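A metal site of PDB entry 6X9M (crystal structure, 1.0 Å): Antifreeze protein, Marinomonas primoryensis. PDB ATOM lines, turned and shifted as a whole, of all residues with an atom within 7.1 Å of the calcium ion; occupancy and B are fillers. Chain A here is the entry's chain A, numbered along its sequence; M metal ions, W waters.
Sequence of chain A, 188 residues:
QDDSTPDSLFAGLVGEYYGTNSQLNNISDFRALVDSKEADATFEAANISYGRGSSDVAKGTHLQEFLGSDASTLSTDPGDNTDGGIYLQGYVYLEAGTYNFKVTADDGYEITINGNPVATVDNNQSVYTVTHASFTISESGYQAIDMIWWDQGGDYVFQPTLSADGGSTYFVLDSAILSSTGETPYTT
N of Gly 60 sits at hydrogen-bond distance from OD1 of Asp 80 (2.8 Å).
OD1 of Asp 77 lies close to NE2 of Gln 64, 3.0 Å away.
Three residues have an atom within 4 Å of the calcium ion: Gly 60, Asp 77 and Pro 78.
The calcium ion is bound by the backbone carbonyl oxygen (O) of Pro 78 (2.3 Å), water W3 (2.4 Å), water W4 (2.4 Å), the backbone carbonyl oxygen (O) of Gly 60 (2.4 Å), water W2 (2.4 Å), water W1 (2.4 Å) and the side-chain carboxylate (OD1) of Asp 77 (2.5 Å).
Water W2 bridges the backbone carbonyl oxygen of Gly 79 (2.8 Å) and the backbone carbonyl oxygen of Ala 58 (3.1 Å).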
ATOM      1  N   VAL A  57      20.741 -28.594  27.061  1.00  0.00           N
ATOM      2  CA  VAL A  57      21.693 -28.000  26.117  1.00  0.00           C
ATOM      3  C   VAL A  57      21.198 -26.667  25.590  1.00  0.00           C
ATOM      4  O   VAL A  57      21.995 -25.802  25.210  1.00  0.00           O
ATOM      5  CB  VAL A  57      22.035 -28.957  24.936  1.00  0.00           C
ATOM      6  CG1 VAL A  57      20.981 -28.892  23.839  1.00  0.00           C
ATOM      7  CG2 VAL A  57      23.408 -28.647  24.385  1.00  0.00           C
ATOM      8  N   ALA A  58      19.869 -26.494  25.521  1.00  0.00           N
ATOM      9  CA  ALA A  58      19.247 -25.371  24.830  1.00  0.00           C
ATOM     10  C   ALA A  58      19.086 -24.149  25.719  1.00  0.00           C
ATOM     11  O   ALA A  58      18.616 -23.108  25.234  1.00  0.00           O
ATOM     12  CB  ALA A  58      17.907 -25.823  24.236  1.00  0.00           C
ATOM     13  N   LYS A  59      19.499 -24.237  26.991  1.00  0.00           N
ATOM     14  CA  LYS A  59      19.415 -23.153  27.952  1.00  0.00           C
ATOM     15  C   LYS A  59      20.732 -22.383  28.068  1.00  0.00           C
ATOM     16  O   LYS A  59      21.812 -22.979  28.024  1.00  0.00           O
ATOM     17  CB  LYS A  59      19.138 -23.725  29.342  1.00  0.00           C
ATOM     18  CG  LYS A  59      17.715 -24.087  29.685  1.00  0.00           C
ATOM     19  CD  LYS A  59      16.947 -24.737  28.595  1.00  0.00           C
ATOM     20  CE  LYS A  59      15.506 -24.767  29.038  1.00  0.00           C
ATOM     21  NZ  LYS A  59      14.923 -23.411  28.899  1.00  0.00           N
ATOM     22  N   GLY A  60      20.630 -21.073  28.299  1.00  0.00           N
ATOM     23  CA  GLY A  60      21.797 -20.304  28.705  1.00  0.00           C
ATOM     24  C   GLY A  60      22.959 -20.486  27.746  1.00  0.00           C
ATOM     25  O   GLY A  60      22.803 -20.417  26.526  1.00  0.00           O
ATOM     26  N   THR A  61      24.141 -20.686  28.319  1.00  0.00           N
ATOM     27  CA  THR A  61      25.369 -20.892  27.561  1.00  0.00           C
ATOM     28  C   THR A  61      25.744 -22.366  27.476  1.00  0.00           C
ATOM     29  O   THR A  61      26.902 -22.698  27.188  1.00  0.00           O
ATOM     30  CB  THR A  61      26.505 -20.057  28.168  1.00  0.00           C
ATOM     31  OG1 THR A  61      26.738 -20.456  29.525  1.00  0.00           O
ATOM     32  CG2 THR A  61      26.160 -18.568  28.160  1.00  0.00           C
ATOM     33  N   HIS A  62      24.775 -23.262  27.690  1.00  0.00           N
ATOM     34  CA  HIS A  62      25.114 -24.685  27.663  1.00  0.00           C
ATOM     35  C   HIS A  62      25.559 -25.148  26.288  1.00  0.00           C
ATOM     36  O   HIS A  62      26.419 -26.026  26.193  1.00  0.00           O
ATOM     37  CB  HIS A  62      23.945 -25.497  28.198  1.00  0.00           C
ATOM     38  CG  HIS A  62      23.654 -25.176  29.635  1.00  0.00           C
ATOM     39  ND1 HIS A  62      22.421 -25.402  30.203  1.00  0.00           N
ATOM     40  CD2 HIS A  62      24.424 -24.639  30.611  1.00  0.00           C
ATOM     41  CE1 HIS A  62      22.439 -24.999  31.464  1.00  0.00           C
ATOM     42  NE2 HIS A  62      23.644 -24.535  31.732  1.00  0.00           N
ATOM     43  N   LEU A  63      24.997 -24.585  25.211  1.00  0.00           N
ATOM     44  CA  LEU A  63      25.434 -24.991  23.878  1.00  0.00           C
ATOM     45  C   LEU A  63      26.892 -24.645  23.644  1.00  0.00           C
ATOM     46  O   LEU A  63      27.655 -25.434  23.092  1.00  0.00           O
ATOM     47  CB  LEU A  63      24.547 -24.352  22.818  1.00  0.00           C
ATOM     48  CG  LEU A  63      24.956 -24.644  21.377  1.00  0.00           C
ATOM     49  CD1 LEU A  63      24.746 -26.115  21.042  1.00  0.00           C
ATOM     50  CD2 LEU A  63      24.160 -23.738  20.426  1.00  0.00           C
ATOM     51  N   GLN A  64      27.293 -23.442  24.072  1.00  0.00           N
ATOM     52  CA  GLN A  64      28.677 -23.018  23.953  1.00  0.00           C
ATOM     53  C   GLN A  64      29.586 -23.982  24.697  1.00  0.00           C
ATOM     54  O   GLN A  64      30.653 -24.367  24.199  1.00  0.00           O
ATOM     55  CB  GLN A  64      28.827 -21.623  24.552  1.00  0.00           C
ATOM     56  CG  GLN A  64      28.332 -20.466  23.730  1.00  0.00           C
ATOM     57  CD  GLN A  64      26.816 -20.232  23.739  1.00  0.00           C
ATOM     58  OE1 GLN A  64      26.039 -20.958  24.367  1.00  0.00           O
ATOM     59  NE2 GLN A  64      26.391 -19.217  23.013  1.00  0.00           N
ATOM     60  N   ASP A  77      24.439 -16.363  19.362  1.00  0.00           N
ATOM     61  CA  ASP A  77      24.133 -17.026  20.622  1.00  0.00           C
ATOM     62  C   ASP A  77      22.630 -17.257  20.673  1.00  0.00           C
ATOM     63  O   ASP A  77      21.873 -16.293  20.864  1.00  0.00           O
ATOM     64  CB  ASP A  77      24.577 -16.145  21.795  1.00  0.00           C
ATOM     65  CG  ASP A  77      24.247 -16.726  23.148  1.00  0.00           C
ATOM     66  OD1 ASP A  77      23.735 -17.877  23.210  1.00  0.00           O
ATOM     67  OD2 ASP A  77      24.507 -16.014  24.158  1.00  0.00           O
ATOM     68  N   PRO A  78      22.144 -18.472  20.467  1.00  0.00           N
ATOM     69  CA  PRO A  78      20.694 -18.706  20.491  1.00  0.00           C
ATOM     70  C   PRO A  78      20.096 -18.298  21.831  1.00  0.00           C
ATOM     71  O   PRO A  78      20.741 -18.395  22.879  1.00  0.00           O
ATOM     72  CB  PRO A  78      20.550 -20.220  20.267  1.00  0.00           C
ATOM     73  CG  PRO A  78      21.841 -20.695  19.759  1.00  0.00           C
ATOM     74  CD  PRO A  78      22.897 -19.722  20.249  1.00  0.00           C
ATOM     75  N   GLY A  79      18.834 -17.893  21.793  1.00  0.00           N
ATOM     76  CA  GLY A  79      18.067 -17.746  23.012  1.00  0.00           C
ATOM     77  C   GLY A  79      17.709 -19.098  23.611  1.00  0.00           C
ATOM     78  O   GLY A  79      18.064 -20.161  23.117  1.00  0.00           O
ATOM     79  N   ASP A  80      17.031 -19.034  24.755  1.00  0.00           N
ATOM     80  CA  ASP A  80      16.689 -20.257  25.470  1.00  0.00           C
ATOM     81  C   ASP A  80      15.610 -21.041  24.725  1.00  0.00           C
ATOM     82  O   ASP A  80      14.662 -20.461  24.167  1.00  0.00           O
ATOM     83  CB  ASP A  80      16.106 -19.940  26.853  1.00  0.00           C
ATOM     84  CG  ASP A  80      17.142 -19.533  27.892  1.00  0.00           C
ATOM     85  OD1 ASP A  80      18.351 -19.562  27.627  1.00  0.00           O
ATOM     86  OD2 ASP A  80      16.663 -19.200  29.016  1.00  0.00           O
HETATM   87 CA    CA M   1      22.094 -19.058  24.656  1.00  0.00          CA
HETATM   88  O   HOH W   1      23.351 -20.875  23.649  1.00  0.00           O
HETATM   89  O   HOH W   2      20.507 -20.867  24.378  1.00  0.00           O
HETATM   90  O   HOH W   3      23.178 -17.467  26.019  1.00  0.00           O
HETATM   91  O   HOH W   4      20.290 -18.295  26.033  1.00  0.00           O
